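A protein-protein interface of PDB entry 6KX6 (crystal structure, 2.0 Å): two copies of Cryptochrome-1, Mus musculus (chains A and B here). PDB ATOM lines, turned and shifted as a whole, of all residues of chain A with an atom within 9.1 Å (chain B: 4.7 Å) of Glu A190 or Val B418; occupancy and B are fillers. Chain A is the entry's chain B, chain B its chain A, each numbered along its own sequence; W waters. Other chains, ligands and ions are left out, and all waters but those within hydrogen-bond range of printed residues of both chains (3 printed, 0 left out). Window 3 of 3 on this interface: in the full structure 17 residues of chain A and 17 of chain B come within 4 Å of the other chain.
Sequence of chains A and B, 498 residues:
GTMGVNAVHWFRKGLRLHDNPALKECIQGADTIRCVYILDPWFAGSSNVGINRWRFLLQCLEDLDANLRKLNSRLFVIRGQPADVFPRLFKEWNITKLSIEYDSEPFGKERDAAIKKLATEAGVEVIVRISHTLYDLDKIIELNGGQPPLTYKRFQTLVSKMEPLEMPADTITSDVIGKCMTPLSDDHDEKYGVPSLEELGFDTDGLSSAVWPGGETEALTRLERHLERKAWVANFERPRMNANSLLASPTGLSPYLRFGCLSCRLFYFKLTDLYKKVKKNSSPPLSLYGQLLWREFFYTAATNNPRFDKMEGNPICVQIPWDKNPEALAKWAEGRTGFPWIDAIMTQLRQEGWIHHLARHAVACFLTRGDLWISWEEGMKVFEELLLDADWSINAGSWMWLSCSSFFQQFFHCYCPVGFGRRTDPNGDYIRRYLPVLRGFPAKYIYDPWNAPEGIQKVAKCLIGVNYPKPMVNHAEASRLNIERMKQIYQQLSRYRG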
ATOM      1  N   ARG A  74      14.109   6.820   6.714  1.00  0.00           N
ATOM      2  CA  ARG A  74      14.991   7.156   7.828  1.00  0.00           C
ATOM      3  C   ARG A  74      16.197   6.228   7.797  1.00  0.00           C
ATOM      4  O   ARG A  74      16.124   5.113   7.274  1.00  0.00           O
ATOM      5  CB  ARG A  74      14.301   7.017   9.196  1.00  0.00           C
ATOM      6  CG  ARG A  74      13.102   7.921   9.439  1.00  0.00           C
ATOM      7  CD  ARG A  74      13.490   9.386   9.516  1.00  0.00           C
ATOM      8  NE  ARG A  74      14.577   9.641  10.455  1.00  0.00           N
ATOM      9  CZ  ARG A  74      14.408   9.829  11.759  1.00  0.00           C
ATOM     10  NH1 ARG A  74      13.193   9.786  12.288  1.00  0.00           N
ATOM     11  NH2 ARG A  74      15.456  10.061  12.538  1.00  0.00           N
ATOM     12  N   VAL A  77      20.222   3.216  12.779  1.00  0.00           N
ATOM     13  CA  VAL A  77      21.517   3.031  13.424  1.00  0.00           C
ATOM     14  C   VAL A  77      21.372   1.966  14.502  1.00  0.00           C
ATOM     15  O   VAL A  77      20.492   2.062  15.366  1.00  0.00           O
ATOM     16  CB  VAL A  77      22.047   4.346  14.018  1.00  0.00           C
ATOM     17  CG1 VAL A  77      23.414   4.126  14.649  1.00  0.00           C
ATOM     18  CG2 VAL A  77      22.120   5.415  12.943  1.00  0.00           C
ATOM     19  N   SER A 185       8.335   3.112  12.849  1.00  0.00           N
ATOM     20  CA  SER A 185       7.595   3.294  14.086  1.00  0.00           C
ATOM     21  C   SER A 185       7.558   4.775  14.447  1.00  0.00           C
ATOM     22  O   SER A 185       8.296   5.593  13.893  1.00  0.00           O
ATOM     23  CB  SER A 185       8.234   2.495  15.223  1.00  0.00           C
ATOM     24  OG  SER A 185       8.719   1.245  14.768  1.00  0.00           O
ATOM     25  N   ASP A 186       6.683   5.122  15.389  1.00  0.00           N
ATOM     26  CA  ASP A 186       6.665   6.489  15.897  1.00  0.00           C
ATOM     27  C   ASP A 186       7.829   6.775  16.836  1.00  0.00           C
ATOM     28  O   ASP A 186       8.211   7.940  16.994  1.00  0.00           O
ATOM     29  CB  ASP A 186       5.344   6.773  16.611  1.00  0.00           C
ATOM     30  CG  ASP A 186       4.380   7.568  15.758  1.00  0.00           C
ATOM     31  OD1 ASP A 186       4.797   8.608  15.202  1.00  0.00           O
ATOM     32  OD2 ASP A 186       3.208   7.156  15.639  1.00  0.00           O
ATOM     33  N   ASP A 187       8.402   5.743  17.449  1.00  0.00           N
ATOM     34  CA  ASP A 187       9.560   5.882  18.329  1.00  0.00           C
ATOM     35  C   ASP A 187      10.857   5.534  17.612  1.00  0.00           C
ATOM     36  O   ASP A 187      11.716   4.849  18.173  1.00  0.00           O
ATOM     37  CB  ASP A 187       9.385   5.013  19.571  1.00  0.00           C
ATOM     38  N   HIS A 188      11.032   5.997  16.371  1.00  0.00           N
ATOM     39  CA  HIS A 188      12.181   5.565  15.582  1.00  0.00           C
ATOM     40  C   HIS A 188      13.487   6.075  16.176  1.00  0.00           C
ATOM     41  O   HIS A 188      14.458   5.321  16.301  1.00  0.00           O
ATOM     42  CB  HIS A 188      12.044   6.028  14.132  1.00  0.00           C
ATOM     43  CG  HIS A 188      13.228   5.686  13.281  1.00  0.00           C
ATOM     44  ND1 HIS A 188      13.331   4.496  12.591  1.00  0.00           N
ATOM     45  CD2 HIS A 188      14.365   6.374  13.014  1.00  0.00           C
ATOM     46  CE1 HIS A 188      14.476   4.468  11.934  1.00  0.00           C
ATOM     47  NE2 HIS A 188      15.122   5.595  12.173  1.00  0.00           N
ATOM     48  N   ASP A 189      13.534   7.361  16.536  1.00  0.00           N
ATOM     49  CA  ASP A 189      14.761   7.924  17.090  1.00  0.00           C
ATOM     50  C   ASP A 189      15.161   7.219  18.379  1.00  0.00           C
ATOM     51  O   ASP A 189      16.351   6.986  18.623  1.00  0.00           O
ATOM     52  CB  ASP A 189      14.591   9.424  17.329  1.00  0.00           C
ATOM     53  CG  ASP A 189      14.501  10.213  16.038  1.00  0.00           C
ATOM     54  OD1 ASP A 189      15.557  10.460  15.415  1.00  0.00           O
ATOM     55  OD2 ASP A 189      13.376  10.587  15.646  1.00  0.00           O
ATOM     56  N   GLU A 190      14.177   6.861  19.209  1.00  0.00           N
ATOM     57  CA  GLU A 190      14.470   6.199  20.477  1.00  0.00           C
ATOM     58  C   GLU A 190      15.180   4.870  20.261  1.00  0.00           C
ATOM     59  O   GLU A 190      16.058   4.492  21.046  1.00  0.00           O
ATOM     60  CB  GLU A 190      13.181   5.987  21.272  1.00  0.00           C
ATOM     61  CG  GLU A 190      12.659   7.229  21.978  1.00  0.00           C
ATOM     62  CD  GLU A 190      11.461   6.938  22.866  1.00  0.00           C
ATOM     63  OE1 GLU A 190      10.976   5.785  22.855  1.00  0.00           O
ATOM     64  OE2 GLU A 190      11.009   7.860  23.579  1.00  0.00           O
ATOM     65  N   LYS A 191      14.812   4.146  19.203  1.00  0.00           N
ATOM     66  CA  LYS A 191      15.374   2.826  18.938  1.00  0.00           C
ATOM     67  C   LYS A 191      16.516   2.844  17.930  1.00  0.00           C
ATOM     68  O   LYS A 191      17.457   2.063  18.069  1.00  0.00           O
ATOM     69  CB  LYS A 191      14.281   1.868  18.448  1.00  0.00           C
ATOM     70  CG  LYS A 191      12.928   2.052  19.130  1.00  0.00           C
ATOM     71  CD  LYS A 191      11.853   1.149  18.541  1.00  0.00           C
ATOM     72  CE  LYS A 191      12.032   0.958  17.048  1.00  0.00           C
ATOM     73  NZ  LYS A 191      11.426   2.067  16.257  1.00  0.00           N
ATOM     74  N   TYR A 192      16.476   3.733  16.933  1.00  0.00           N
ATOM     75  CA  TYR A 192      17.428   3.681  15.829  1.00  0.00           C
ATOM     76  C   TYR A 192      18.084   5.024  15.524  1.00  0.00           C
ATOM     77  O   TYR A 192      18.708   5.163  14.464  1.00  0.00           O
ATOM     78  CB  TYR A 192      16.745   3.161  14.558  1.00  0.00           C
ATOM     79  CG  TYR A 192      16.165   1.765  14.665  1.00  0.00           C
ATOM     80  CD1 TYR A 192      16.989   0.658  14.820  1.00  0.00           C
ATOM     81  CD2 TYR A 192      14.791   1.557  14.586  1.00  0.00           C
ATOM     82  CE1 TYR A 192      16.463  -0.621  14.908  1.00  0.00           C
ATOM     83  CE2 TYR A 192      14.256   0.283  14.668  1.00  0.00           C
ATOM     84  CZ  TYR A 192      15.095  -0.802  14.834  1.00  0.00           C
ATOM     85  OH  TYR A 192      14.566  -2.068  14.922  1.00  0.00           O
ATOM     86  N   GLY A 193      17.963   6.012  16.407  1.00  0.00           N
ATOM     87  CA  GLY A 193      18.489   7.330  16.111  1.00  0.00           C
ATOM     88  C   GLY A 193      20.007   7.380  16.094  1.00  0.00           C
ATOM     89  O   GLY A 193      20.704   6.530  16.651  1.00  0.00           O
ATOM     90  N   VAL A 194      20.524   8.410  15.434  1.00  0.00           N
ATOM     91  CA  VAL A 194      21.970   8.658  15.459  1.00  0.00           C
ATOM     92  C   VAL A 194      22.356   9.189  16.835  1.00  0.00           C
ATOM     93  O   VAL A 194      21.754  10.169  17.310  1.00  0.00           O
ATOM     94  CB  VAL A 194      22.363   9.649  14.364  1.00  0.00           C
ATOM     95  CG1 VAL A 194      23.870   9.848  14.358  1.00  0.00           C
ATOM     96  CG2 VAL A 194      21.877   9.166  13.008  1.00  0.00           C
ATOM     97  N   PRO A 195      23.327   8.590  17.511  1.00  0.00           N
ATOM     98  CA  PRO A 195      23.693   9.060  18.847  1.00  0.00           C
ATOM     99  C   PRO A 195      24.648  10.241  18.780  1.00  0.00           C
ATOM    100  O   PRO A 195      25.296  10.501  17.765  1.00  0.00           O
ATOM    101  CB  PRO A 195      24.370   7.836  19.469  1.00  0.00           C
ATOM    102  CG  PRO A 195      25.013   7.161  18.296  1.00  0.00           C
ATOM    103  CD  PRO A 195      24.110   7.410  17.106  1.00  0.00           C
ATOM    104  N   GLU A 199      26.551  10.392  24.111  1.00  0.00           N
ATOM    105  CA  GLU A 199      25.832   9.129  24.192  1.00  0.00           C
ATOM    106  C   GLU A 199      26.741   7.939  23.917  1.00  0.00           C
ATOM    107  O   GLU A 199      26.412   6.818  24.319  1.00  0.00           O
ATOM    108  CB  GLU A 199      24.637   9.143  23.236  1.00  0.00           C
ATOM    109  CG  GLU A 199      23.372   9.700  23.890  1.00  0.00           C
ATOM    110  CD  GLU A 199      22.440  10.397  22.920  1.00  0.00           C
ATOM    111  OE1 GLU A 199      22.921  11.219  22.111  1.00  0.00           O
ATOM    112  OE2 GLU A 199      21.219  10.136  22.986  1.00  0.00           O
ATOM    113  N   PHE B 339      10.486   9.053  32.900  1.00  0.00           N
ATOM    114  CA  PHE B 339      11.611   8.539  32.135  1.00  0.00           C
ATOM    115  C   PHE B 339      12.582   7.879  33.101  1.00  0.00           C
ATOM    116  O   PHE B 339      13.238   8.587  33.880  1.00  0.00           O
ATOM    117  CB  PHE B 339      12.299   9.666  31.366  1.00  0.00           C
ATOM    118  CG  PHE B 339      11.495  10.183  30.202  1.00  0.00           C
ATOM    119  CD1 PHE B 339      10.524  11.155  30.387  1.00  0.00           C
ATOM    120  CD2 PHE B 339      11.710   9.693  28.924  1.00  0.00           C
ATOM    121  CE1 PHE B 339       9.787  11.632  29.313  1.00  0.00           C
ATOM    122  CE2 PHE B 339      10.976  10.163  27.847  1.00  0.00           C
ATOM    123  CZ  PHE B 339      10.014  11.133  28.042  1.00  0.00           C
ATOM    124  N   CYS B 416      18.854  11.809  24.142  1.00  0.00           N
ATOM    125  CA  CYS B 416      17.567  11.126  24.229  1.00  0.00           C
ATOM    126  C   CYS B 416      17.387  10.555  25.631  1.00  0.00           C
ATOM    127  O   CYS B 416      18.261   9.829  26.110  1.00  0.00           O
ATOM    128  CB  CYS B 416      17.474  10.009  23.201  1.00  0.00           C
ATOM    129  SG  CYS B 416      15.957   9.030  23.258  1.00  0.00           S
ATOM    130  N   PRO B 417      16.283  10.867  26.317  1.00  0.00           N
ATOM    131  CA  PRO B 417      16.096  10.366  27.689  1.00  0.00           C
ATOM    132  C   PRO B 417      15.783   8.880  27.757  1.00  0.00           C
ATOM    133  O   PRO B 417      15.701   8.336  28.866  1.00  0.00           O
ATOM    134  CB  PRO B 417      14.928  11.208  28.211  1.00  0.00           C
ATOM    135  CG  PRO B 417      14.140  11.534  26.990  1.00  0.00           C
ATOM    136  CD  PRO B 417      15.164  11.729  25.894  1.00  0.00           C
ATOM    137  N   VAL B 418      15.589   8.221  26.621  1.00  0.00           N
ATOM    138  CA  VAL B 418      15.506   6.767  26.558  1.00  0.00           C
ATOM    139  C   VAL B 418      16.808   6.167  26.050  1.00  0.00           C
ATOM    140  O   VAL B 418      17.381   5.278  26.681  1.00  0.00           O
ATOM    141  CB  VAL B 418      14.310   6.334  25.680  1.00  0.00           C
ATOM    142  CG1 VAL B 418      14.439   4.867  25.276  1.00  0.00           C
ATOM    143  CG2 VAL B 418      12.997   6.583  26.409  1.00  0.00           C
ATOM    144  N   GLY B 419      17.313   6.682  24.927  1.00  0.00           N
ATOM    145  CA  GLY B 419      18.454   6.057  24.276  1.00  0.00           C
ATOM    146  C   GLY B 419      19.754   6.185  25.051  1.00  0.00           C
ATOM    147  O   GLY B 419      20.569   5.259  25.059  1.00  0.00           O
ATOM    148  N   PHE B 420      19.979   7.334  25.696  1.00  0.00           N
ATOM    149  CA  PHE B 420      21.253   7.551  26.381  1.00  0.00           C
ATOM    150  C   PHE B 420      21.469   6.513  27.477  1.00  0.00           C
ATOM    151  O   PHE B 420      22.540   5.902  27.567  1.00  0.00           O
ATOM    152  CB  PHE B 420      21.321   8.971  26.953  1.00  0.00           C
ATOM    153  CG  PHE B 420      22.715   9.405  27.358  1.00  0.00           C
ATOM    154  CD1 PHE B 420      23.812   8.581  27.141  1.00  0.00           C
ATOM    155  CD2 PHE B 420      22.928  10.640  27.945  1.00  0.00           C
ATOM    156  CE1 PHE B 420      25.085   8.974  27.515  1.00  0.00           C
ATOM    157  CE2 PHE B 420      24.206  11.041  28.314  1.00  0.00           C
ATOM    158  CZ  PHE B 420      25.283  10.204  28.095  1.00  0.00           C
ATOM    159  N   GLY B 421      20.458   6.297  28.320  1.00  0.00           N
ATOM    160  CA  GLY B 421      20.579   5.267  29.337  1.00  0.00           C
ATOM    161  C   GLY B 421      20.758   3.884  28.738  1.00  0.00           C
ATOM    162  O   GLY B 421      21.618   3.112  29.170  1.00  0.00           O
ATOM    163  N   ARG B 422      19.949   3.561  27.725  1.00  0.00           N
ATOM    164  CA  ARG B 422      20.028   2.250  27.089  1.00  0.00           C
ATOM    165  C   ARG B 422      21.411   2.001  26.502  1.00  0.00           C
ATOM    166  O   ARG B 422      21.918   0.875  26.546  1.00  0.00           O
ATOM    167  CB  ARG B 422      18.951   2.138  26.009  1.00  0.00           C
ATOM    168  CG  ARG B 422      18.781   0.754  25.402  1.00  0.00           C
ATOM    169  CD  ARG B 422      17.694   0.784  24.338  1.00  0.00           C
ATOM    170  NE  ARG B 422      16.356   0.780  24.924  1.00  0.00           N
ATOM    171  CZ  ARG B 422      15.308   1.419  24.413  1.00  0.00           C
ATOM    172  NH1 ARG B 422      15.432   2.131  23.300  1.00  0.00           N
ATOM    173  NH2 ARG B 422      14.132   1.350  25.022  1.00  0.00           N
ATOM    174  N   TYR B 447      13.945   0.953  30.055  1.00  0.00           N
ATOM    175  CA  TYR B 447      14.128   2.375  29.803  1.00  0.00           C
ATOM    176  C   TYR B 447      12.903   3.040  29.191  1.00  0.00           C
ATOM    177  O   TYR B 447      12.828   4.272  29.183  1.00  0.00           O
ATOM    178  CB  TYR B 447      15.344   2.588  28.897  1.00  0.00           C
ATOM    179  CG  TYR B 447      16.653   2.323  29.600  1.00  0.00           C
ATOM    180  CD1 TYR B 447      17.195   3.260  30.472  1.00  0.00           C
ATOM    181  CD2 TYR B 447      17.340   1.132  29.407  1.00  0.00           C
ATOM    182  CE1 TYR B 447      18.390   3.023  31.123  1.00  0.00           C
ATOM    183  CE2 TYR B 447      18.538   0.885  30.056  1.00  0.00           C
ATOM    184  CZ  TYR B 447      19.057   1.837  30.912  1.00  0.00           C
ATOM    185  OH  TYR B 447      20.247   1.601  31.562  1.00  0.00           O
ATOM    186  N   ASP B 448      11.945   2.264  28.687  1.00  0.00           N
ATOM    187  CA  ASP B 448      10.687   2.796  28.158  1.00  0.00           C
ATOM    188  C   ASP B 448       9.554   1.869  28.579  1.00  0.00           C
ATOM    189  O   ASP B 448       8.923   1.206  27.747  1.00  0.00           O
ATOM    190  CB  ASP B 448      10.755   2.950  26.637  1.00  0.00           C
ATOM    191  CG  ASP B 448      11.162   1.666  25.932  1.00  0.00           C
ATOM    192  OD1 ASP B 448      11.845   0.829  26.560  1.00  0.00           O
ATOM    193  OD2 ASP B 448      10.801   1.495  24.748  1.00  0.00           O
ATOM    194  N   TRP B 450       6.555   2.273  29.415  1.00  0.00           N
ATOM    195  CA  TRP B 450       5.233   2.516  28.851  1.00  0.00           C
ATOM    196  C   TRP B 450       4.994   1.701  27.587  1.00  0.00           C
ATOM    197  O   TRP B 450       3.836   1.492  27.210  1.00  0.00           O
ATOM    198  CB  TRP B 450       5.050   4.003  28.555  1.00  0.00           C
ATOM    199  CG  TRP B 450       6.086   4.563  27.626  1.00  0.00           C
ATOM    200  CD1 TRP B 450       6.033   4.593  26.261  1.00  0.00           C
ATOM    201  CD2 TRP B 450       7.329   5.175  27.992  1.00  0.00           C
ATOM    202  NE1 TRP B 450       7.165   5.184  25.756  1.00  0.00           N
ATOM    203  CE2 TRP B 450       7.976   5.553  26.798  1.00  0.00           C
ATOM    204  CE3 TRP B 450       7.958   5.443  29.214  1.00  0.00           C
ATOM    205  CZ2 TRP B 450       9.220   6.182  26.788  1.00  0.00           C
ATOM    206  CZ3 TRP B 450       9.191   6.068  29.204  1.00  0.00           C
ATOM    207  CH2 TRP B 450       9.811   6.431  27.998  1.00  0.00           C
ATOM    208  N   ASN B 451       6.058   1.237  26.929  1.00  0.00           N
ATOM    209  CA  ASN B 451       5.921   0.406  25.740  1.00  0.00           C
ATOM    210  C   ASN B 451       5.687  -1.062  26.063  1.00  0.00           C
ATOM    211  O   ASN B 451       5.431  -1.844  25.141  1.00  0.00           O
ATOM    212  CB  ASN B 451       7.166   0.527  24.854  1.00  0.00           C
ATOM    213  CG  ASN B 451       7.225   1.840  24.102  1.00  0.00           C
ATOM    214  OD1 ASN B 451       6.194   2.423  23.760  1.00  0.00           O
ATOM    215  ND2 ASN B 451       8.438   2.315  23.838  1.00  0.00           N
HETATM  216  O   HOH W   1      18.240   2.895  21.955  1.00  0.00           O
HETATM  217  O   HOH W   2       8.235   5.363  23.197  1.00  0.00           O
HETATM  218  O   HOH W   3      11.890   2.810  22.948  1.00  0.00           O
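The side-chain carboxylate (OE2) of Glu A199 sits at hydrogen-bond distance from the backbone NH (N) of Cys B416 (3.1 Å).
The backbone carbonyl oxygen (O) of Glu A190 is in hydrogen-bond range of the guanidinium group (NH1) of Arg B422 (3.3 Å).
The side-chain sulfur (SG) of Cys B416 lies close to the backbone NH (N) of Val B418 (3.5 Å).
The side-chain sulfur (SG) of Cys B416 is in hydrogen-bond range of the backbone NH (N) of Gly B419 (3.2 Å).
NH2 of Arg B422 is in salt-bridge range of OD1 of Asp B448 (2.8 Å).
Among the printed residues, pairs that only touch across the chains: Glu A190 with Cys B416 (3.97 Å), Glu A190 with Val B418 (3.7 Å) and Glu A199 with Phe B420 (3.4 Å).
Glu A190 touches three residues of chain B.
Val A194 touches none of the printed residues of chain B.
Of the printed residues of chain B, Glu A199 touches Cys B416 (3.1 Å) and Phe B420 (3.4 Å).
Printed residues of chain A within 4 Å of Cys B416: Glu A190 and Glu A199.
Of the printed residues of chain A, Val B418 touches Glu A190 (3.7 Å).
No residue of chain A comes within 4 Å of Gly B419.
Of the printed residues of chain A, Phe B420 touches Glu A199.
Of the printed residues of chain A, Arg B422 touches Glu A190.
The nearest residue of chain B that does not touch Glu A190 is Trp B450 (4.04 Å).
The nearest residue of chain A that does not touch Val B418 is Lys A191 (6.1 Å).
The nearest printed residue of chain A that does not touch Cys B416 is Asp A189 (5.1 Å).
Along chain A the printed residues that touch a printed residue of chain B span positions 190 to 199.
Of the 12 printed residues of chain B, 4 touch a printed residue of chain A.
Hydrophobic or aromatic side chains of chain B that line the printed part of chain A: Val B418 and Phe B420.
Among the printed residues, 5 pairs touch across the chains.
No position is printed for both chains.
Water W3 lies within hydrogen-bond range of the side-chain carboxylate (OD2) of Asp B448, the side-chain carboxylate (OE1) of Glu A190 and the guanidinium group (NH2) of Arg B422.
Water W2 lies within hydrogen-bond range of NE1 of Trp B450 (2.8 Å), OE1 of Glu A190 (2.8 Å) and ND2 of Asn B451 (3.1 Å).
Water W1 bridges O of Glu A190 and NH1 of Arg B422.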
